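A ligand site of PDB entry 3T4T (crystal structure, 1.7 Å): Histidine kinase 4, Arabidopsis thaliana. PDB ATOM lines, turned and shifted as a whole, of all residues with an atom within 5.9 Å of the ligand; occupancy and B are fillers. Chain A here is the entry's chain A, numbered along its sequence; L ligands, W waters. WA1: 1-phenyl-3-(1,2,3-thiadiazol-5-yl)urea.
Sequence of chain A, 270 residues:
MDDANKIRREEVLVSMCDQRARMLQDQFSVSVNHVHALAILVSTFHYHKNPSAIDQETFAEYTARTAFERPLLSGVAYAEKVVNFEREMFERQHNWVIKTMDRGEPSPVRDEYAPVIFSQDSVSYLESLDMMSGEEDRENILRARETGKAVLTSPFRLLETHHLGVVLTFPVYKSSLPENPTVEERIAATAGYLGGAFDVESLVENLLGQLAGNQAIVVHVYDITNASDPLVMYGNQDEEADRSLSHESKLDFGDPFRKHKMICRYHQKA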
ATOM      1  N   ALA A  77     -11.503  20.233 -16.235  1.00  0.00           N
ATOM      2  CA  ALA A  77     -12.004  19.834 -14.947  1.00  0.00           C
ATOM      3  C   ALA A  77     -13.425  20.337 -14.801  1.00  0.00           C
ATOM      4  O   ALA A  77     -13.842  21.298 -15.479  1.00  0.00           O
ATOM      5  CB  ALA A  77     -11.099  20.415 -13.856  1.00  0.00           C
ATOM      6  N   TYR A  78     -14.140  19.740 -13.866  1.00  0.00           N
ATOM      7  CA  TYR A  78     -15.508  20.140 -13.532  1.00  0.00           C
ATOM      8  C   TYR A  78     -15.560  20.539 -12.044  1.00  0.00           C
ATOM      9  O   TYR A  78     -15.187  19.761 -11.182  1.00  0.00           O
ATOM     10  CB  TYR A  78     -16.491  19.015 -13.812  1.00  0.00           C
ATOM     11  CG  TYR A  78     -17.858  19.427 -13.408  1.00  0.00           C
ATOM     12  CD1 TYR A  78     -18.554  20.380 -14.163  1.00  0.00           C
ATOM     13  CD2 TYR A  78     -18.436  18.952 -12.237  1.00  0.00           C
ATOM     14  CE1 TYR A  78     -19.834  20.845 -13.747  1.00  0.00           C
ATOM     15  CE2 TYR A  78     -19.732  19.441 -11.822  1.00  0.00           C
ATOM     16  CZ  TYR A  78     -20.376  20.370 -12.585  1.00  0.00           C
ATOM     17  OH  TYR A  78     -21.613  20.880 -12.223  1.00  0.00           O
ATOM     18  N   ALA A  79     -16.072  21.762 -11.794  1.00  0.00           N
ATOM     19  CA  ALA A  79     -16.221  22.330 -10.456  1.00  0.00           C
ATOM     20  C   ALA A  79     -17.703  22.449 -10.167  1.00  0.00           C
ATOM     21  O   ALA A  79     -18.464  22.868 -11.036  1.00  0.00           O
ATOM     22  CB  ALA A  79     -15.567  23.675 -10.340  1.00  0.00           C
ATOM     23  N   MET A 101      -6.855  27.942  -3.707  1.00  0.00           N
ATOM     24  CA  MET A 101      -5.963  27.559  -4.797  1.00  0.00           C
ATOM     25  C   MET A 101      -4.566  28.090  -4.593  1.00  0.00           C
ATOM     26  O   MET A 101      -3.610  27.572  -5.188  1.00  0.00           O
ATOM     27  CB  MET A 101      -6.493  28.001  -6.153  1.00  0.00           C
ATOM     28  CG  MET A 101      -6.278  29.403  -6.460  1.00  0.00           C
ATOM     29  SD  MET A 101      -6.715  29.776  -8.153  1.00  0.00           S
ATOM     30  CE  MET A 101      -8.277  28.907  -8.313  1.00  0.00           C
ATOM     31  N   VAL A 116     -13.363  21.858  -7.415  1.00  0.00           N
ATOM     32  CA  VAL A 116     -13.201  20.868  -8.473  1.00  0.00           C
ATOM     33  C   VAL A 116     -13.460  19.453  -7.932  1.00  0.00           C
ATOM     34  O   VAL A 116     -12.817  19.015  -6.973  1.00  0.00           O
ATOM     35  CB  VAL A 116     -11.816  20.971  -9.090  1.00  0.00           C
ATOM     36  CG1 VAL A 116     -11.545  19.724 -10.062  1.00  0.00           C
ATOM     37  CG2 VAL A 116     -11.698  22.280  -9.838  1.00  0.00           C
ATOM     38  N   VAL A 123      -4.270  17.759 -14.805  1.00  0.00           N
ATOM     39  CA  VAL A 123      -4.536  18.863 -13.822  1.00  0.00           C
ATOM     40  C   VAL A 123      -5.123  18.308 -12.525  1.00  0.00           C
ATOM     41  O   VAL A 123      -6.002  18.899 -11.895  1.00  0.00           O
ATOM     42  CB  VAL A 123      -5.403  19.959 -14.448  1.00  0.00           C
ATOM     43  CG1 VAL A 123      -4.637  20.717 -15.512  1.00  0.00           C
ATOM     44  CG2 VAL A 123      -6.747  19.426 -15.002  1.00  0.00           C
ATOM     45  N   TYR A 125      -3.970  18.138  -9.596  1.00  0.00           N
ATOM     46  CA  TYR A 125      -3.740  19.085  -8.489  1.00  0.00           C
ATOM     47  C   TYR A 125      -4.922  20.027  -8.252  1.00  0.00           C
ATOM     48  O   TYR A 125      -5.016  20.641  -7.159  1.00  0.00           O
ATOM     49  CB  TYR A 125      -2.484  19.916  -8.696  1.00  0.00           C
ATOM     50  CG  TYR A 125      -2.322  20.514 -10.068  1.00  0.00           C
ATOM     51  CD1 TYR A 125      -2.965  21.692 -10.435  1.00  0.00           C
ATOM     52  CD2 TYR A 125      -1.536  19.872 -11.040  1.00  0.00           C
ATOM     53  CE1 TYR A 125      -2.828  22.242 -11.711  1.00  0.00           C
ATOM     54  CE2 TYR A 125      -1.371  20.425 -12.314  1.00  0.00           C
ATOM     55  CZ  TYR A 125      -2.022  21.589 -12.647  1.00  0.00           C
ATOM     56  OH  TYR A 125      -1.854  22.109 -13.909  1.00  0.00           O
ATOM     57  N   LEU A 126      -5.849  20.144  -9.216  1.00  0.00           N
ATOM     58  CA  LEU A 126      -7.029  21.000  -8.998  1.00  0.00           C
ATOM     59  C   LEU A 126      -8.066  20.366  -8.091  1.00  0.00           C
ATOM     60  O   LEU A 126      -8.921  21.065  -7.539  1.00  0.00           O
ATOM     61  CB  LEU A 126      -7.705  21.367 -10.313  1.00  0.00           C
ATOM     62  CG  LEU A 126      -6.868  22.159 -11.307  1.00  0.00           C
ATOM     63  CD1 LEU A 126      -7.556  22.222 -12.684  1.00  0.00           C
ATOM     64  CD2 LEU A 126      -6.562  23.562 -10.769  1.00  0.00           C
ATOM     65  N   MET A 131     -12.274  27.116  -7.247  1.00  0.00           N
ATOM     66  CA  MET A 131     -11.945  27.908  -8.409  1.00  0.00           C
ATOM     67  C   MET A 131     -12.365  29.374  -8.255  1.00  0.00           C
ATOM     68  O   MET A 131     -11.899  30.218  -8.996  1.00  0.00           O
ATOM     69  CB  MET A 131     -12.498  27.290  -9.708  1.00  0.00           C
ATOM     70  CG  MET A 131     -11.929  25.904 -10.066  1.00  0.00           C
ATOM     71  SD  MET A 131     -10.160  25.900 -10.340  1.00  0.00           S
ATOM     72  CE  MET A 131      -9.603  25.399  -8.774  1.00  0.00           C
ATOM     73  N   ASP A 137     -10.206  33.262 -12.358  1.00  0.00           N
ATOM     74  CA  ASP A 137     -11.157  32.152 -12.393  1.00  0.00           C
ATOM     75  C   ASP A 137     -12.521  32.556 -11.821  1.00  0.00           C
ATOM     76  O   ASP A 137     -13.548  32.252 -12.426  1.00  0.00           O
ATOM     77  CB  ASP A 137     -10.608  30.948 -11.662  1.00  0.00           C
ATOM     78  CG  ASP A 137      -9.827  30.010 -12.585  1.00  0.00           C
ATOM     79  OD1 ASP A 137     -10.460  29.555 -13.558  1.00  0.00           O
ATOM     80  OD2 ASP A 137      -8.644  29.718 -12.329  1.00  0.00           O
ATOM     81  N   ILE A 141     -16.000  32.525 -13.867  1.00  0.00           N
ATOM     82  CA  ILE A 141     -17.130  31.733 -13.361  1.00  0.00           C
ATOM     83  C   ILE A 141     -18.416  32.576 -13.353  1.00  0.00           C
ATOM     84  O   ILE A 141     -19.485  32.137 -13.794  1.00  0.00           O
ATOM     85  CB  ILE A 141     -16.805  31.096 -11.980  1.00  0.00           C
ATOM     86  CG1 ILE A 141     -15.998  29.788 -12.176  1.00  0.00           C
ATOM     87  CG2 ILE A 141     -18.076  30.794 -11.201  1.00  0.00           C
ATOM     88  CD1 ILE A 141     -15.195  29.343 -10.952  1.00  0.00           C
ATOM     89  N   PHE A 156      -2.909  35.003 -17.599  1.00  0.00           N
ATOM     90  CA  PHE A 156      -2.251  34.925 -16.294  1.00  0.00           C
ATOM     91  C   PHE A 156      -1.421  33.655 -16.159  1.00  0.00           C
ATOM     92  O   PHE A 156      -1.518  32.752 -16.990  1.00  0.00           O
ATOM     93  CB  PHE A 156      -3.293  35.048 -15.166  1.00  0.00           C
ATOM     94  CG  PHE A 156      -4.180  33.853 -14.983  1.00  0.00           C
ATOM     95  CD1 PHE A 156      -5.260  33.599 -15.822  1.00  0.00           C
ATOM     96  CD2 PHE A 156      -3.976  32.981 -13.919  1.00  0.00           C
ATOM     97  CE1 PHE A 156      -6.086  32.507 -15.634  1.00  0.00           C
ATOM     98  CE2 PHE A 156      -4.785  31.875 -13.742  1.00  0.00           C
ATOM     99  CZ  PHE A 156      -5.821  31.625 -14.595  1.00  0.00           C
ATOM    100  N   ARG A 157      -0.576  33.604 -15.130  1.00  0.00           N
ATOM    101  CA  ARG A 157       0.284  32.451 -14.945  1.00  0.00           C
ATOM    102  C   ARG A 157      -0.506  31.352 -14.239  1.00  0.00           C
ATOM    103  O   ARG A 157      -0.975  31.506 -13.095  1.00  0.00           O
ATOM    104  CB  ARG A 157       1.598  32.813 -14.245  1.00  0.00           C
ATOM    105  CG  ARG A 157       2.467  33.718 -15.132  1.00  0.00           C
ATOM    106  CD  ARG A 157       3.954  33.650 -14.835  1.00  0.00           C
ATOM    107  NE  ARG A 157       4.725  34.441 -15.805  1.00  0.00           N
ATOM    108  CZ  ARG A 157       5.214  34.006 -16.969  1.00  0.00           C
ATOM    109  NH1 ARG A 157       5.042  32.730 -17.364  1.00  0.00           N
ATOM    110  NH2 ARG A 157       5.883  34.836 -17.754  1.00  0.00           N
ATOM    111  N   LEU A 158      -0.677  30.245 -14.957  1.00  0.00           N
ATOM    112  CA  LEU A 158      -1.473  29.106 -14.524  1.00  0.00           C
ATOM    113  C   LEU A 158      -0.895  28.452 -13.277  1.00  0.00           C
ATOM    114  O   LEU A 158       0.290  28.517 -12.999  1.00  0.00           O
ATOM    115  CB  LEU A 158      -1.601  28.075 -15.666  1.00  0.00           C
ATOM    116  CG  LEU A 158      -2.303  28.554 -16.953  1.00  0.00           C
ATOM    117  CD1 LEU A 158      -2.388  27.443 -17.994  1.00  0.00           C
ATOM    118  CD2 LEU A 158      -3.717  29.101 -16.661  1.00  0.00           C
ATOM    119  N   LEU A 159      -1.770  27.805 -12.526  1.00  0.00           N
ATOM    120  CA  LEU A 159      -1.379  27.060 -11.344  1.00  0.00           C
ATOM    121  C   LEU A 159      -0.335  26.000 -11.684  1.00  0.00           C
ATOM    122  O   LEU A 159      -0.384  25.389 -12.758  1.00  0.00           O
ATOM    123  CB  LEU A 159      -2.613  26.406 -10.740  1.00  0.00           C
ATOM    124  CG  LEU A 159      -3.578  27.370 -10.078  1.00  0.00           C
ATOM    125  CD1 LEU A 159      -4.870  26.629  -9.779  1.00  0.00           C
ATOM    126  CD2 LEU A 159      -2.941  27.959  -8.825  1.00  0.00           C
ATOM    127  N   VAL A 167      -7.864  30.689 -19.089  1.00  0.00           N
ATOM    128  CA  VAL A 167      -8.826  29.662 -18.759  1.00  0.00           C
ATOM    129  C   VAL A 167     -10.122  29.925 -19.498  1.00  0.00           C
ATOM    130  O   VAL A 167     -10.595  31.084 -19.616  1.00  0.00           O
ATOM    131  CB  VAL A 167      -9.112  29.630 -17.234  1.00  0.00           C
ATOM    132  CG1 VAL A 167     -10.310  28.722 -16.942  1.00  0.00           C
ATOM    133  CG2 VAL A 167      -7.865  29.141 -16.518  1.00  0.00           C
ATOM    134  N   LEU A 168     -10.711  28.845 -19.988  1.00  0.00           N
ATOM    135  CA  LEU A 168     -12.009  28.842 -20.666  1.00  0.00           C
ATOM    136  C   LEU A 168     -12.981  28.177 -19.720  1.00  0.00           C
ATOM    137  O   LEU A 168     -12.680  27.103 -19.184  1.00  0.00           O
ATOM    138  CB  LEU A 168     -11.926  28.022 -21.942  1.00  0.00           C
ATOM    139  CG  LEU A 168     -13.231  27.658 -22.671  1.00  0.00           C
ATOM    140  CD1 LEU A 168     -13.768  28.879 -23.389  1.00  0.00           C
ATOM    141  CD2 LEU A 168     -13.037  26.511 -23.693  1.00  0.00           C
ATOM    142  N   THR A 169     -14.155  28.787 -19.487  1.00  0.00           N
ATOM    143  CA  THR A 169     -15.135  28.256 -18.505  1.00  0.00           C
ATOM    144  C   THR A 169     -16.519  28.245 -19.171  1.00  0.00           C
ATOM    145  O   THR A 169     -16.892  29.210 -19.881  1.00  0.00           O
ATOM    146  CB  THR A 169     -15.128  29.096 -17.223  1.00  0.00           C
ATOM    147  OG1 THR A 169     -13.791  29.174 -16.692  1.00  0.00           O
ATOM    148  CG2 THR A 169     -16.099  28.488 -16.166  1.00  0.00           C
ATOM    149  N   TYR A 193     -19.421  24.291 -13.273  1.00  0.00           N
ATOM    150  CA  TYR A 193     -18.629  24.904 -14.319  1.00  0.00           C
ATOM    151  C   TYR A 193     -17.619  23.923 -14.897  1.00  0.00           C
ATOM    152  O   TYR A 193     -16.946  23.222 -14.136  1.00  0.00           O
ATOM    153  CB  TYR A 193     -17.846  26.107 -13.721  1.00  0.00           C
ATOM    154  CG  TYR A 193     -18.662  26.853 -12.658  1.00  0.00           C
ATOM    155  CD1 TYR A 193     -19.628  27.768 -13.049  1.00  0.00           C
ATOM    156  CD2 TYR A 193     -18.515  26.574 -11.308  1.00  0.00           C
ATOM    157  CE1 TYR A 193     -20.418  28.406 -12.107  1.00  0.00           C
ATOM    158  CE2 TYR A 193     -19.291  27.205 -10.370  1.00  0.00           C
ATOM    159  CZ  TYR A 193     -20.228  28.123 -10.777  1.00  0.00           C
ATOM    160  OH  TYR A 193     -21.021  28.777  -9.823  1.00  0.00           O
ATOM    161  N   LEU A 194     -17.499  23.915 -16.226  1.00  0.00           N
ATOM    162  CA  LEU A 194     -16.509  23.097 -16.931  1.00  0.00           C
ATOM    163  C   LEU A 194     -15.399  24.051 -17.356  1.00  0.00           C
ATOM    164  O   LEU A 194     -15.631  25.001 -18.120  1.00  0.00           O
ATOM    165  CB  LEU A 194     -17.125  22.402 -18.137  1.00  0.00           C
ATOM    166  CG  LEU A 194     -16.466  21.111 -18.592  1.00  0.00           C
ATOM    167  CD1 LEU A 194     -14.939  21.291 -18.892  1.00  0.00           C
ATOM    168  CD2 LEU A 194     -16.595  20.005 -17.541  1.00  0.00           C
ATOM    169  N   GLY A 195     -14.215  23.840 -16.798  1.00  0.00           N
ATOM    170  CA  GLY A 195     -13.074  24.694 -17.025  1.00  0.00           C
ATOM    171  C   GLY A 195     -11.983  23.988 -17.797  1.00  0.00           C
ATOM    172  O   GLY A 195     -11.724  22.776 -17.595  1.00  0.00           O
ATOM    173  N   GLY A 196     -11.367  24.731 -18.715  1.00  0.00           N
ATOM    174  CA  GLY A 196     -10.269  24.194 -19.497  1.00  0.00           C
ATOM    175  C   GLY A 196      -9.116  25.171 -19.444  1.00  0.00           C
ATOM    176  O   GLY A 196      -9.311  26.355 -19.699  1.00  0.00           O
ATOM    177  N   ALA A 197      -7.925  24.662 -19.125  1.00  0.00           N
ATOM    178  CA  ALA A 197      -6.711  25.464 -19.093  1.00  0.00           C
ATOM    179  C   ALA A 197      -5.996  25.509 -20.450  1.00  0.00           C
ATOM    180  O   ALA A 197      -5.521  24.476 -20.938  1.00  0.00           O
ATOM    181  CB  ALA A 197      -5.779  24.912 -18.058  1.00  0.00           C
HETATM  182  OAA WA1 L   1      -8.755  25.042 -14.137  1.00  0.00           O
HETATM  183  CAB WA1 L   1     -13.945  24.634 -13.571  1.00  0.00           C
HETATM  184  CAC WA1 L   1     -12.766  23.944 -13.470  1.00  0.00           C
HETATM  185  CAD WA1 L   1     -13.922  26.018 -13.753  1.00  0.00           C
HETATM  186  CAE WA1 L   1     -11.554  24.595 -13.520  1.00  0.00           C
HETATM  187  CAF WA1 L   1     -12.736  26.650 -13.817  1.00  0.00           C
HETATM  188  CAG WA1 L   1      -5.718  27.907 -13.313  1.00  0.00           C
HETATM  189  NAH WA1 L   1      -4.554  27.303 -13.402  1.00  0.00           N
HETATM  190  NAI WA1 L   1      -4.601  26.064 -13.997  1.00  0.00           N
HETATM  191  NAJ WA1 L   1     -10.350  26.713 -13.718  1.00  0.00           N
HETATM  192  NAK WA1 L   1      -8.117  27.266 -13.591  1.00  0.00           N
HETATM  193  SAL WA1 L   1      -6.130  25.525 -14.250  1.00  0.00           S
HETATM  194  CAM WA1 L   1      -9.040  26.220 -13.814  1.00  0.00           C
HETATM  195  CAN WA1 L   1     -11.537  25.991 -13.736  1.00  0.00           C
HETATM  196  CAO WA1 L   1      -6.758  27.069 -13.640  1.00  0.00           C
HETATM  197  O   HOH W   1      -8.969  22.920 -16.036  1.00  0.00           O
HETATM  198  O   HOH W   2     -13.074  30.060 -14.285  1.00  0.00           O
HETATM  199  O   HOH W   3      -2.331  24.470 -14.409  1.00  0.00           O
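N of Gly 195 sits at hydrogen-bond distance from O of Ala 77.
The backbone carbonyl oxygen (O) of Ala 79 lies within hydrogen-bond range of the backbone NH (N) of Tyr 193 (2.8 Å).
The side-chain carboxylate (OD2) of Asp 137 lies within hydrogen-bond range of a nitrogen (NAK) of the ligand, 2.8 Å away.
The backbone NH (N) of Leu 159 sits at hydrogen-bond distance from a nitrogen (NAH) of the ligand, 3.0 Å away.
The side-chain sulfur of Met 131 sits at hydrogen-bond distance from a nitrogen (NAJ) of the ligand, at 3.5 Å.
Water W3 lies within hydrogen-bond range of OH of Tyr 125 (2.5 Å), O of Leu 159 (2.7 Å) and NAI of the ligand (2.8 Å).
Water W1 bridges OAA of the ligand (2.9 Å) and O of Gly 195 (3.2 Å).
Water W2 bridges the side-chain hydroxyl (OG1) of Thr 169 (2.7 Å) and the side-chain carboxylate (OD1) of Asp 137 (2.8 Å).
O of Ala 77 touches CAC of the ligand, at 3.5 Å.
CB of Ala 79 touches CAB of the ligand, at 3.7 Å.
Leu 126 touches the ligand (CD1 to OAA, 3.4 Å).
Phe 156 touches the ligand.
CA of Leu 158 touches NAH of the ligand, 3.7 Å away.
Val 167 touches the ligand (CG2 to NAK, 3.5 Å).
Thr 169 touches the ligand (OG1 to CAF, 3.97 Å).
Tyr 193 touches the ligand (O to CAB, 3.4 Å).
Gly 195 touches the ligand (N to CAB, 3.3 Å).
Ala 197 touches the ligand.
13 residues have an atom within 4 Å of the ligand: Ala 77, Ala 79, Leu 126, Met 131, Asp 137, Phe 156, Leu 158, Leu 159, Val 167, Thr 169, Tyr 193, Gly 195 and Ala 197.
The nearest printed residue that does not touch the ligand is Leu 194 (4.1 Å).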
